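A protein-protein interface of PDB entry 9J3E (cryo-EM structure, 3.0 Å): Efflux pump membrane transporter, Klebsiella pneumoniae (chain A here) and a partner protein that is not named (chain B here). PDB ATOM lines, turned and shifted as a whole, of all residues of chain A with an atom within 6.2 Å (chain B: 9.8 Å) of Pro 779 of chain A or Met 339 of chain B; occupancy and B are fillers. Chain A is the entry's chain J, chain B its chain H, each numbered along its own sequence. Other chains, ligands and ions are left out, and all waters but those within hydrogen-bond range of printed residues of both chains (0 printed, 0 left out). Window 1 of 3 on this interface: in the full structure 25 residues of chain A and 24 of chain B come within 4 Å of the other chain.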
ATOM      1  N   LEU A 723     -12.412 -16.765  19.197  1.00  0.00           N
ATOM      2  CA  LEU A 723     -12.608 -15.530  18.452  1.00  0.00           C
ATOM      3  C   LEU A 723     -14.058 -15.501  17.986  1.00  0.00           C
ATOM      4  O   LEU A 723     -14.380 -15.973  16.899  1.00  0.00           O
ATOM      5  CB  LEU A 723     -11.632 -15.452  17.288  1.00  0.00           C
ATOM      6  CG  LEU A 723     -11.345 -14.107  16.622  1.00  0.00           C
ATOM      7  CD1 LEU A 723     -10.207 -14.272  15.652  1.00  0.00           C
ATOM      8  CD2 LEU A 723     -12.541 -13.596  15.893  1.00  0.00           C
ATOM      9  N   PHE A 750     -12.592 -21.421   5.947  1.00  0.00           N
ATOM     10  CA  PHE A 750     -11.823 -21.798   7.123  1.00  0.00           C
ATOM     11  C   PHE A 750     -12.077 -23.216   7.598  1.00  0.00           C
ATOM     12  O   PHE A 750     -11.152 -23.867   8.082  1.00  0.00           O
ATOM     13  CB  PHE A 750     -12.088 -20.815   8.266  1.00  0.00           C
ATOM     14  CG  PHE A 750     -11.439 -19.478   8.069  1.00  0.00           C
ATOM     15  CD1 PHE A 750     -10.165 -19.243   8.539  1.00  0.00           C
ATOM     16  CD2 PHE A 750     -12.086 -18.469   7.391  1.00  0.00           C
ATOM     17  CE1 PHE A 750      -9.563 -18.023   8.362  1.00  0.00           C
ATOM     18  CE2 PHE A 750     -11.479 -17.247   7.204  1.00  0.00           C
ATOM     19  CZ  PHE A 750     -10.215 -17.029   7.685  1.00  0.00           C
ATOM     20  N   MET A 777      -4.223 -17.612   8.143  1.00  0.00           N
ATOM     21  CA  MET A 777      -3.362 -17.766   9.302  1.00  0.00           C
ATOM     22  C   MET A 777      -3.608 -16.719  10.372  1.00  0.00           C
ATOM     23  O   MET A 777      -2.955 -16.764  11.416  1.00  0.00           O
ATOM     24  CB  MET A 777      -1.891 -17.704   8.895  1.00  0.00           C
ATOM     25  CG  MET A 777      -1.235 -18.975   8.329  1.00  0.00           C
ATOM     26  SD  MET A 777      -1.350 -20.573   9.169  1.00  0.00           S
ATOM     27  CE  MET A 777      -3.049 -21.065   8.899  1.00  0.00           C
ATOM     28  N   THR A 778      -4.496 -15.768  10.140  1.00  0.00           N
ATOM     29  CA  THR A 778      -4.578 -14.584  10.976  1.00  0.00           C
ATOM     30  C   THR A 778      -6.020 -14.134  11.136  1.00  0.00           C
ATOM     31  O   THR A 778      -6.830 -14.286  10.218  1.00  0.00           O
ATOM     32  CB  THR A 778      -3.707 -13.484  10.345  1.00  0.00           C
ATOM     33  OG1 THR A 778      -2.342 -13.688  10.726  1.00  0.00           O
ATOM     34  CG2 THR A 778      -4.131 -12.103  10.748  1.00  0.00           C
ATOM     35  N   PRO A 779      -6.382 -13.594  12.304  1.00  0.00           N
ATOM     36  CA  PRO A 779      -7.751 -13.089  12.477  1.00  0.00           C
ATOM     37  C   PRO A 779      -8.137 -12.046  11.457  1.00  0.00           C
ATOM     38  O   PRO A 779      -9.295 -12.011  11.025  1.00  0.00           O
ATOM     39  CB  PRO A 779      -7.723 -12.493  13.889  1.00  0.00           C
ATOM     40  CG  PRO A 779      -6.657 -13.231  14.580  1.00  0.00           C
ATOM     41  CD  PRO A 779      -5.607 -13.504  13.550  1.00  0.00           C
ATOM     42  N   GLU A 780      -7.198 -11.192  11.055  1.00  0.00           N
ATOM     43  CA  GLU A 780      -7.476 -10.213  10.015  1.00  0.00           C
ATOM     44  C   GLU A 780      -7.850 -10.886   8.706  1.00  0.00           C
ATOM     45  O   GLU A 780      -8.589 -10.310   7.900  1.00  0.00           O
ATOM     46  CB  GLU A 780      -6.262  -9.308   9.816  1.00  0.00           C
ATOM     47  CG  GLU A 780      -5.884  -8.457  11.022  1.00  0.00           C
ATOM     48  CD  GLU A 780      -5.189  -9.237  12.122  1.00  0.00           C
ATOM     49  OE1 GLU A 780      -5.770 -10.224  12.618  1.00  0.00           O
ATOM     50  OE2 GLU A 780      -4.053  -8.871  12.487  1.00  0.00           O
ATOM     51  N   SER A 781      -7.362 -12.106   8.481  1.00  0.00           N
ATOM     52  CA  SER A 781      -7.730 -12.825   7.271  1.00  0.00           C
ATOM     53  C   SER A 781      -9.205 -13.187   7.267  1.00  0.00           C
ATOM     54  O   SER A 781      -9.815 -13.290   6.197  1.00  0.00           O
ATOM     55  CB  SER A 781      -6.873 -14.073   7.125  1.00  0.00           C
ATOM     56  OG  SER A 781      -5.583 -13.845   7.652  1.00  0.00           O
ATOM     57  N   VAL A 782      -9.797 -13.391   8.443  1.00  0.00           N
ATOM     58  CA  VAL A 782     -11.239 -13.596   8.507  1.00  0.00           C
ATOM     59  C   VAL A 782     -11.952 -12.377   7.953  1.00  0.00           C
ATOM     60  O   VAL A 782     -12.891 -12.486   7.160  1.00  0.00           O
ATOM     61  CB  VAL A 782     -11.682 -13.885   9.951  1.00  0.00           C
ATOM     62  CG1 VAL A 782     -13.193 -13.830  10.059  1.00  0.00           C
ATOM     63  CG2 VAL A 782     -11.151 -15.217  10.415  1.00  0.00           C
ATOM     64  N   LEU A 783     -11.502 -11.193   8.356  1.00  0.00           N
ATOM     65  CA  LEU A 783     -12.113  -9.969   7.876  1.00  0.00           C
ATOM     66  C   LEU A 783     -11.852  -9.738   6.397  1.00  0.00           C
ATOM     67  O   LEU A 783     -12.703  -9.162   5.714  1.00  0.00           O
ATOM     68  CB  LEU A 783     -11.603  -8.776   8.680  1.00  0.00           C
ATOM     69  CG  LEU A 783     -12.014  -8.697  10.150  1.00  0.00           C
ATOM     70  CD1 LEU A 783     -13.413  -9.244  10.346  1.00  0.00           C
ATOM     71  CD2 LEU A 783     -11.017  -9.400  11.047  1.00  0.00           C
ATOM     72  N   ARG A 784     -10.703 -10.162   5.889  1.00  0.00           N
ATOM     73  CA  ARG A 784     -10.384  -9.907   4.494  1.00  0.00           C
ATOM     74  C   ARG A 784     -11.222 -10.730   3.533  1.00  0.00           C
ATOM     75  O   ARG A 784     -11.198 -10.457   2.331  1.00  0.00           O
ATOM     76  CB  ARG A 784      -8.905 -10.169   4.233  1.00  0.00           C
ATOM     77  CG  ARG A 784      -7.997  -9.051   4.683  1.00  0.00           C
ATOM     78  CD  ARG A 784      -6.587  -9.328   4.237  1.00  0.00           C
ATOM     79  NE  ARG A 784      -5.971 -10.365   5.052  1.00  0.00           N
ATOM     80  CZ  ARG A 784      -5.073 -11.229   4.606  1.00  0.00           C
ATOM     81  NH1 ARG A 784      -4.686 -11.232   3.342  1.00  0.00           N
ATOM     82  NH2 ARG A 784      -4.557 -12.120   5.446  1.00  0.00           N
ATOM     83  N   THR A 803     -14.532  -8.670  15.386  1.00  0.00           N
ATOM     84  CA  THR A 803     -13.970  -9.807  16.093  1.00  0.00           C
ATOM     85  C   THR A 803     -13.807  -9.458  17.560  1.00  0.00           C
ATOM     86  O   THR A 803     -13.097  -8.507  17.901  1.00  0.00           O
ATOM     87  CB  THR A 803     -12.619 -10.196  15.503  1.00  0.00           C
ATOM     88  OG1 THR A 803     -11.707  -9.102  15.648  1.00  0.00           O
ATOM     89  CG2 THR A 803     -12.769 -10.541  14.036  1.00  0.00           C
ATOM     90  N   TRP A 805     -12.728 -11.315  21.226  1.00  0.00           N
ATOM     91  CA  TRP A 805     -12.123 -12.500  21.805  1.00  0.00           C
ATOM     92  C   TRP A 805     -12.909 -12.943  23.025  1.00  0.00           C
ATOM     93  O   TRP A 805     -13.492 -12.123  23.736  1.00  0.00           O
ATOM     94  CB  TRP A 805     -10.673 -12.227  22.187  1.00  0.00           C
ATOM     95  CG  TRP A 805      -9.757 -12.245  21.023  1.00  0.00           C
ATOM     96  CD1 TRP A 805      -9.321 -11.176  20.306  1.00  0.00           C
ATOM     97  CD2 TRP A 805      -9.156 -13.396  20.432  1.00  0.00           C
ATOM     98  NE1 TRP A 805      -8.485 -11.589  19.303  1.00  0.00           N
ATOM     99  CE2 TRP A 805      -8.366 -12.951  19.362  1.00  0.00           C
ATOM    100  CE3 TRP A 805      -9.204 -14.759  20.711  1.00  0.00           C
ATOM    101  CZ2 TRP A 805      -7.637 -13.819  18.569  1.00  0.00           C
ATOM    102  CZ3 TRP A 805      -8.483 -15.617  19.925  1.00  0.00           C
ATOM    103  CH2 TRP A 805      -7.707 -15.148  18.866  1.00  0.00           C
ATOM    104  N   PHE B  49       7.241   0.208  13.564  1.00  0.00           N
ATOM    105  CA  PHE B  49       6.505  -0.840  12.870  1.00  0.00           C
ATOM    106  C   PHE B  49       5.307  -0.214  12.183  1.00  0.00           C
ATOM    107  O   PHE B  49       4.428   0.339  12.848  1.00  0.00           O
ATOM    108  CB  PHE B  49       6.059  -1.932  13.841  1.00  0.00           C
ATOM    109  CG  PHE B  49       5.224  -3.001  13.214  1.00  0.00           C
ATOM    110  CD1 PHE B  49       5.708  -3.745  12.156  1.00  0.00           C
ATOM    111  CD2 PHE B  49       3.950  -3.263  13.685  1.00  0.00           C
ATOM    112  CE1 PHE B  49       4.939  -4.734  11.582  1.00  0.00           C
ATOM    113  CE2 PHE B  49       3.176  -4.248  13.115  1.00  0.00           C
ATOM    114  CZ  PHE B  49       3.670  -4.985  12.062  1.00  0.00           C
ATOM    115  N   THR B  50       5.275  -0.304  10.861  1.00  0.00           N
ATOM    116  CA  THR B  50       4.192   0.243  10.059  1.00  0.00           C
ATOM    117  C   THR B  50       3.271  -0.893   9.648  1.00  0.00           C
ATOM    118  O   THR B  50       3.727  -1.888   9.077  1.00  0.00           O
ATOM    119  CB  THR B  50       4.737   0.958   8.826  1.00  0.00           C
ATOM    120  OG1 THR B  50       5.608   2.020   9.230  1.00  0.00           O
ATOM    121  CG2 THR B  50       3.601   1.530   8.002  1.00  0.00           C
ATOM    122  N   VAL B  51       1.986  -0.753   9.945  1.00  0.00           N
ATOM    123  CA  VAL B  51       1.005  -1.757   9.553  1.00  0.00           C
ATOM    124  C   VAL B  51       0.605  -1.517   8.106  1.00  0.00           C
ATOM    125  O   VAL B  51       0.161  -0.422   7.746  1.00  0.00           O
ATOM    126  CB  VAL B  51      -0.215  -1.714  10.482  1.00  0.00           C
ATOM    127  CG1 VAL B  51      -1.227  -2.758  10.067  1.00  0.00           C
ATOM    128  CG2 VAL B  51       0.217  -1.932  11.914  1.00  0.00           C
ATOM    129  N   PHE B  52       0.756  -2.539   7.275  1.00  0.00           N
ATOM    130  CA  PHE B  52       0.482  -2.437   5.850  1.00  0.00           C
ATOM    131  C   PHE B  52      -0.738  -3.276   5.518  1.00  0.00           C
ATOM    132  O   PHE B  52      -0.862  -4.408   5.992  1.00  0.00           O
ATOM    133  CB  PHE B  52       1.679  -2.909   5.028  1.00  0.00           C
ATOM    134  CG  PHE B  52       2.853  -1.985   5.087  1.00  0.00           C
ATOM    135  CD1 PHE B  52       2.946  -0.905   4.234  1.00  0.00           C
ATOM    136  CD2 PHE B  52       3.871  -2.202   5.996  1.00  0.00           C
ATOM    137  CE1 PHE B  52       4.028  -0.057   4.290  1.00  0.00           C
ATOM    138  CE2 PHE B  52       4.954  -1.356   6.058  1.00  0.00           C
ATOM    139  CZ  PHE B  52       5.033  -0.283   5.203  1.00  0.00           C
ATOM    140  N   ILE B 303       5.779  -2.302  19.969  1.00  0.00           N
ATOM    141  CA  ILE B 303       6.358  -3.399  20.728  1.00  0.00           C
ATOM    142  C   ILE B 303       5.759  -4.697  20.215  1.00  0.00           C
ATOM    143  O   ILE B 303       4.534  -4.864  20.209  1.00  0.00           O
ATOM    144  CB  ILE B 303       6.103  -3.233  22.230  1.00  0.00           C
ATOM    145  CG1 ILE B 303       7.045  -2.182  22.804  1.00  0.00           C
ATOM    146  CG2 ILE B 303       6.270  -4.553  22.936  1.00  0.00           C
ATOM    147  CD1 ILE B 303       6.695  -1.756  24.199  1.00  0.00           C
ATOM    148  N   LEU B 304       6.614  -5.616  19.786  1.00  0.00           N
ATOM    149  CA  LEU B 304       6.186  -6.929  19.333  1.00  0.00           C
ATOM    150  C   LEU B 304       6.716  -7.977  20.298  1.00  0.00           C
ATOM    151  O   LEU B 304       7.884  -7.926  20.692  1.00  0.00           O
ATOM    152  CB  LEU B 304       6.674  -7.215  17.913  1.00  0.00           C
ATOM    153  CG  LEU B 304       6.317  -6.175  16.854  1.00  0.00           C
ATOM    154  CD1 LEU B 304       6.504  -6.745  15.469  1.00  0.00           C
ATOM    155  CD2 LEU B 304       4.900  -5.702  17.028  1.00  0.00           C
ATOM    156  N   VAL B 305       5.855  -8.908  20.691  1.00  0.00           N
ATOM    157  CA  VAL B 305       6.258  -9.987  21.586  1.00  0.00           C
ATOM    158  C   VAL B 305       5.848 -11.302  20.943  1.00  0.00           C
ATOM    159  O   VAL B 305       4.910 -11.322  20.137  1.00  0.00           O
ATOM    160  CB  VAL B 305       5.624  -9.835  22.975  1.00  0.00           C
ATOM    161  CG1 VAL B 305       6.117  -8.571  23.648  1.00  0.00           C
ATOM    162  CG2 VAL B 305       4.119  -9.853  22.870  1.00  0.00           C
ATOM    163  N   PRO B 306       6.511 -12.411  21.250  1.00  0.00           N
ATOM    164  CA  PRO B 306       6.123 -13.682  20.644  1.00  0.00           C
ATOM    165  C   PRO B 306       4.691 -14.042  20.994  1.00  0.00           C
ATOM    166  O   PRO B 306       4.221 -13.799  22.106  1.00  0.00           O
ATOM    167  CB  PRO B 306       7.114 -14.680  21.245  1.00  0.00           C
ATOM    168  CG  PRO B 306       8.269 -13.861  21.647  1.00  0.00           C
ATOM    169  CD  PRO B 306       7.707 -12.554  22.091  1.00  0.00           C
ATOM    170  N   GLN B 307       4.004 -14.638  20.025  1.00  0.00           N
ATOM    171  CA  GLN B 307       2.613 -15.018  20.217  1.00  0.00           C
ATOM    172  C   GLN B 307       2.448 -16.032  21.330  1.00  0.00           C
ATOM    173  O   GLN B 307       1.369 -16.140  21.921  1.00  0.00           O
ATOM    174  CB  GLN B 307       2.067 -15.594  18.927  1.00  0.00           C
ATOM    175  CG  GLN B 307       0.658 -15.272  18.707  1.00  0.00           C
ATOM    176  CD  GLN B 307       0.380 -14.978  17.274  1.00  0.00           C
ATOM    177  OE1 GLN B 307       1.288 -14.944  16.442  1.00  0.00           O
ATOM    178  NE2 GLN B 307      -0.885 -14.777  16.961  1.00  0.00           N
ATOM    179  N   ARG B 308       3.498 -16.795  21.610  1.00  0.00           N
ATOM    180  CA  ARG B 308       3.451 -17.777  22.676  1.00  0.00           C
ATOM    181  C   ARG B 308       3.297 -17.126  24.038  1.00  0.00           C
ATOM    182  O   ARG B 308       2.812 -17.775  24.969  1.00  0.00           O
ATOM    183  CB  ARG B 308       4.725 -18.606  22.640  1.00  0.00           C
ATOM    184  CG  ARG B 308       4.642 -19.849  21.800  1.00  0.00           C
ATOM    185  CD  ARG B 308       5.921 -19.984  21.008  1.00  0.00           C
ATOM    186  NE  ARG B 308       7.016 -20.469  21.832  1.00  0.00           N
ATOM    187  CZ  ARG B 308       7.770 -21.515  21.532  1.00  0.00           C
ATOM    188  NH1 ARG B 308       7.591 -22.198  20.414  1.00  0.00           N
ATOM    189  NH2 ARG B 308       8.734 -21.880  22.372  1.00  0.00           N
ATOM    190  N   VAL B 310       1.415 -14.584  25.104  1.00  0.00           N
ATOM    191  CA  VAL B 310       0.174 -13.863  25.364  1.00  0.00           C
ATOM    192  C   VAL B 310      -0.849 -14.847  25.909  1.00  0.00           C
ATOM    193  O   VAL B 310      -1.084 -15.903  25.312  1.00  0.00           O
ATOM    194  CB  VAL B 310      -0.355 -13.167  24.105  1.00  0.00           C
ATOM    195  CG1 VAL B 310      -1.725 -12.583  24.371  1.00  0.00           C
ATOM    196  CG2 VAL B 310       0.604 -12.082  23.669  1.00  0.00           C
ATOM    197  N   ARG B 312      -4.956 -15.157  27.520  1.00  0.00           N
ATOM    198  CA  ARG B 312      -6.257 -14.504  27.498  1.00  0.00           C
ATOM    199  C   ARG B 312      -7.133 -15.062  28.606  1.00  0.00           C
ATOM    200  O   ARG B 312      -7.202 -16.278  28.797  1.00  0.00           O
ATOM    201  CB  ARG B 312      -6.949 -14.670  26.148  1.00  0.00           C
ATOM    202  CG  ARG B 312      -6.328 -13.843  25.049  1.00  0.00           C
ATOM    203  CD  ARG B 312      -7.281 -13.667  23.889  1.00  0.00           C
ATOM    204  NE  ARG B 312      -6.702 -12.822  22.853  1.00  0.00           N
ATOM    205  CZ  ARG B 312      -6.865 -11.510  22.791  1.00  0.00           C
ATOM    206  NH1 ARG B 312      -7.608 -10.866  23.674  1.00  0.00           N
ATOM    207  NH2 ARG B 312      -6.272 -10.827  21.820  1.00  0.00           N
ATOM    208  N   THR B 336      -3.988  -6.321  22.933  1.00  0.00           N
ATOM    209  CA  THR B 336      -3.256  -6.796  21.775  1.00  0.00           C
ATOM    210  C   THR B 336      -3.781  -6.129  20.513  1.00  0.00           C
ATOM    211  O   THR B 336      -4.977  -5.875  20.391  1.00  0.00           O
ATOM    212  CB  THR B 336      -3.362  -8.315  21.695  1.00  0.00           C
ATOM    213  OG1 THR B 336      -4.542  -8.663  20.953  1.00  0.00           O
ATOM    214  CG2 THR B 336      -3.438  -8.915  23.081  1.00  0.00           C
ATOM    215  N   GLY B 337      -2.876  -5.838  19.584  1.00  0.00           N
ATOM    216  CA  GLY B 337      -3.234  -5.143  18.360  1.00  0.00           C
ATOM    217  C   GLY B 337      -3.397  -6.043  17.153  1.00  0.00           C
ATOM    218  O   GLY B 337      -4.444  -6.670  16.989  1.00  0.00           O
ATOM    219  N   ALA B 338      -2.403  -6.099  16.278  1.00  0.00           N
ATOM    220  CA  ALA B 338      -2.473  -7.014  15.153  1.00  0.00           C
ATOM    221  C   ALA B 338      -1.355  -8.040  15.239  1.00  0.00           C
ATOM    222  O   ALA B 338      -0.506  -8.010  16.133  1.00  0.00           O
ATOM    223  CB  ALA B 338      -2.415  -6.265  13.822  1.00  0.00           C
ATOM    224  N   MET B 339      -1.382  -8.967  14.295  1.00  0.00           N
ATOM    225  CA  MET B 339      -0.459 -10.087  14.235  1.00  0.00           C
ATOM    226  C   MET B 339       0.497  -9.907  13.070  1.00  0.00           C
ATOM    227  O   MET B 339       0.061  -9.744  11.927  1.00  0.00           O
ATOM    228  CB  MET B 339      -1.232 -11.389  14.079  1.00  0.00           C
ATOM    229  CG  MET B 339      -2.317 -11.565  15.107  1.00  0.00           C
ATOM    230  SD  MET B 339      -2.461 -13.292  15.573  1.00  0.00           S
ATOM    231  CE  MET B 339      -1.710 -14.056  14.137  1.00  0.00           C
ATOM    232  N   GLN B 340       1.790  -9.942  13.359  1.00  0.00           N
ATOM    233  CA  GLN B 340       2.830  -9.814  12.344  1.00  0.00           C
ATOM    234  C   GLN B 340       3.713 -11.049  12.438  1.00  0.00           C
ATOM    235  O   GLN B 340       4.601 -11.127  13.291  1.00  0.00           O
ATOM    236  CB  GLN B 340       3.640  -8.538  12.536  1.00  0.00           C
ATOM    237  CG  GLN B 340       4.765  -8.334  11.524  1.00  0.00           C
ATOM    238  CD  GLN B 340       4.436  -8.878  10.145  1.00  0.00           C
ATOM    239  OE1 GLN B 340       4.807  -9.999   9.800  1.00  0.00           O
ATOM    240  NE2 GLN B 340       3.745  -8.077   9.345  1.00  0.00           N
ATOM    241  N   GLY B 341       3.475 -12.007  11.553  1.00  0.00           N
ATOM    242  CA  GLY B 341       4.224 -13.240  11.592  1.00  0.00           C
ATOM    243  C   GLY B 341       3.911 -14.035  12.838  1.00  0.00           C
ATOM    244  O   GLY B 341       2.764 -14.430  13.053  1.00  0.00           O
ATOM    245  N   SER B 342       4.919 -14.272  13.673  1.00  0.00           N
ATOM    246  CA  SER B 342       4.743 -15.057  14.886  1.00  0.00           C
ATOM    247  C   SER B 342       4.539 -14.193  16.116  1.00  0.00           C
ATOM    248  O   SER B 342       4.398 -14.726  17.218  1.00  0.00           O
ATOM    249  CB  SER B 342       5.947 -15.968  15.107  1.00  0.00           C
ATOM    250  OG  SER B 342       7.128 -15.200  15.230  1.00  0.00           O
ATOM    251  N   ARG B 343       4.511 -12.878  15.960  1.00  0.00           N
ATOM    252  CA  ARG B 343       4.550 -11.963  17.085  1.00  0.00           C
ATOM    253  C   ARG B 343       3.291 -11.121  17.077  1.00  0.00           C
ATOM    254  O   ARG B 343       2.720 -10.861  16.015  1.00  0.00           O
ATOM    255  CB  ARG B 343       5.783 -11.075  17.011  1.00  0.00           C
ATOM    256  CG  ARG B 343       7.080 -11.814  17.180  1.00  0.00           C
ATOM    257  CD  ARG B 343       8.197 -10.819  17.191  1.00  0.00           C
ATOM    258  NE  ARG B 343       8.313 -10.213  15.873  1.00  0.00           N
ATOM    259  CZ  ARG B 343       8.928  -9.069  15.622  1.00  0.00           C
ATOM    260  NH1 ARG B 343       9.503  -8.368  16.583  1.00  0.00           N
ATOM    261  NH2 ARG B 343       8.958  -8.611  14.374  1.00  0.00           N
ATOM    262  N   TRP B 344       2.844 -10.713  18.251  1.00  0.00           N
ATOM    263  CA  TRP B 344       1.664  -9.883  18.299  1.00  0.00           C
ATOM    264  C   TRP B 344       2.132  -8.438  18.307  1.00  0.00           C
ATOM    265  O   TRP B 344       3.266  -8.150  18.693  1.00  0.00           O
ATOM    266  CB  TRP B 344       0.851 -10.127  19.555  1.00  0.00           C
ATOM    267  CG  TRP B 344      -0.331 -10.910  19.286  1.00  0.00           C
ATOM    268  CD1 TRP B 344      -0.351 -12.247  19.122  1.00  0.00           C
ATOM    269  CD2 TRP B 344      -1.599 -10.443  18.844  1.00  0.00           C
ATOM    270  NE1 TRP B 344      -1.603 -12.671  18.795  1.00  0.00           N
ATOM    271  CE2 TRP B 344      -2.389 -11.574  18.588  1.00  0.00           C
ATOM    272  CE3 TRP B 344      -2.170  -9.186  18.714  1.00  0.00           C
ATOM    273  CZ2 TRP B 344      -3.714 -11.484  18.202  1.00  0.00           C
ATOM    274  CZ3 TRP B 344      -3.487  -9.100  18.328  1.00  0.00           C
ATOM    275  CH2 TRP B 344      -4.242 -10.239  18.081  1.00  0.00           C
ATOM    276  N   GLN B 345       1.266  -7.523  17.904  1.00  0.00           N
ATOM    277  CA  GLN B 345       1.540  -6.122  18.175  1.00  0.00           C
ATOM    278  C   GLN B 345       0.802  -5.708  19.435  1.00  0.00           C
ATOM    279  O   GLN B 345      -0.428  -5.775  19.493  1.00  0.00           O
ATOM    280  CB  GLN B 345       1.119  -5.234  17.010  1.00  0.00           C
ATOM    281  CG  GLN B 345       1.361  -3.765  17.288  1.00  0.00           C
ATOM    282  CD  GLN B 345       0.603  -2.854  16.354  1.00  0.00           C
ATOM    283  OE1 GLN B 345      -0.344  -3.275  15.698  1.00  0.00           O
ATOM    284  NE2 GLN B 345       1.017  -1.594  16.286  1.00  0.00           N
ATOM    285  N   ILE B 346       1.550  -5.281  20.445  1.00  0.00           N
ATOM    286  CA  ILE B 346       0.978  -4.880  21.723  1.00  0.00           C
ATOM    287  C   ILE B 346       0.718  -3.384  21.673  1.00  0.00           C
ATOM    288  O   ILE B 346       1.620  -2.598  21.358  1.00  0.00           O
ATOM    289  CB  ILE B 346       1.891  -5.251  22.898  1.00  0.00           C
ATOM    290  CG1 ILE B 346       1.582  -6.665  23.398  1.00  0.00           C
ATOM    291  CG2 ILE B 346       1.725  -4.258  24.024  1.00  0.00           C
ATOM    292  CD1 ILE B 346       1.449  -7.707  22.326  1.00  0.00           C
ATOM    293  N   SER B 347      -0.515  -2.989  21.970  1.00  0.00           N
ATOM    294  CA  SER B 347      -0.877  -1.582  21.923  1.00  0.00           C
ATOM    295  C   SER B 347      -0.680  -0.873  23.254  1.00  0.00           C
ATOM    296  O   SER B 347      -0.348   0.317  23.266  1.00  0.00           O
ATOM    297  CB  SER B 347      -2.330  -1.430  21.475  1.00  0.00           C
ATOM    298  OG  SER B 347      -3.197  -2.135  22.340  1.00  0.00           O
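NE1 of Trp 805 of chain A sits close to NH2 of Arg 312 of chain B, at 3.4 Å.
The side-chain carboxylate (OE2) of Glu 780 of chain A lies within hydrogen-bond range of the backbone NH (N) of Met 339 of chain B.
The side-chain sulfur (SD) of Met 339 of chain B is in hydrogen-bond range of the side-chain amide nitrogen (NE2) of Gln 307 of chain B, at 2.6 Å.
The backbone carbonyl oxygen (O) of Thr 778 of chain A is in hydrogen-bond range of the side-chain hydroxyl (OG) of Ser 781 of chain A, at 2.9 Å.
The backbone carbonyl oxygen of Ala 338 of chain B is in hydrogen-bond range of the backbone NH of Gln 345 of chain B (2.6 Å).
The guanidinium group of Arg 312 of chain B lies within hydrogen-bond range of the side-chain hydroxyl of Thr 336 of chain B (2.9 Å).
The indole nitrogen (NE1) of Trp 344 of chain B is in hydrogen-bond range of the side-chain sulfur (SD) of Met 339 of chain B (3.4 Å).
Among the printed residues, pairs that only touch across the chains: Thr 778 of chain A with Met 339 of chain B (3.5 Å), Pro 779 of chain A with Met 339 of chain B (3.7 Å) and Glu 780 of chain A with Ala 338 of chain B (3.4 Å).
Of the printed residues of chain B, Thr 778 of chain A touches Met 339 (3.5 Å).
Printed residues of chain B within 4 Å of Glu 780 of chain A: Ala 338 (3.4 Å) and Met 339 (3.2 Å).
Printed residues of chain B within 4 Å of Trp 805 of chain A: Arg 312.
Phe 52 of chain B touches none of the printed residues of chain A.
Of the printed residues of chain A, Arg 312 of chain B touches Trp 805 (3.4 Å).
Printed residues of chain A within 4 Å of Ala 338 of chain B: Glu 780.
Met 339 of chain B touches just these residues of chain A: Thr 778 (3.5 Å), Pro 779 (3.7 Å) and Glu 780 (3.2 Å).
The nearest residue of chain A that does not touch Met 339 of chain B is Met 777 of chain A (4.04 Å).
Of the 24 printed residues of chain B, 3 touch a printed residue of chain A.
Hydrophobic or aromatic side chains of chain B that line the printed part of chain A: Ala 338 and Met 339.
Of the 12 printed residues of chain A, 4 touch a printed residue of chain B.
Hydrophobic or aromatic side chains of chain A that line the printed part of chain B: Pro 779 and Trp 805.
Among the printed residues, no Asp or Glu carboxylate lies within 4 Å of a Lys or Arg side-chain nitrogen of the other chain.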
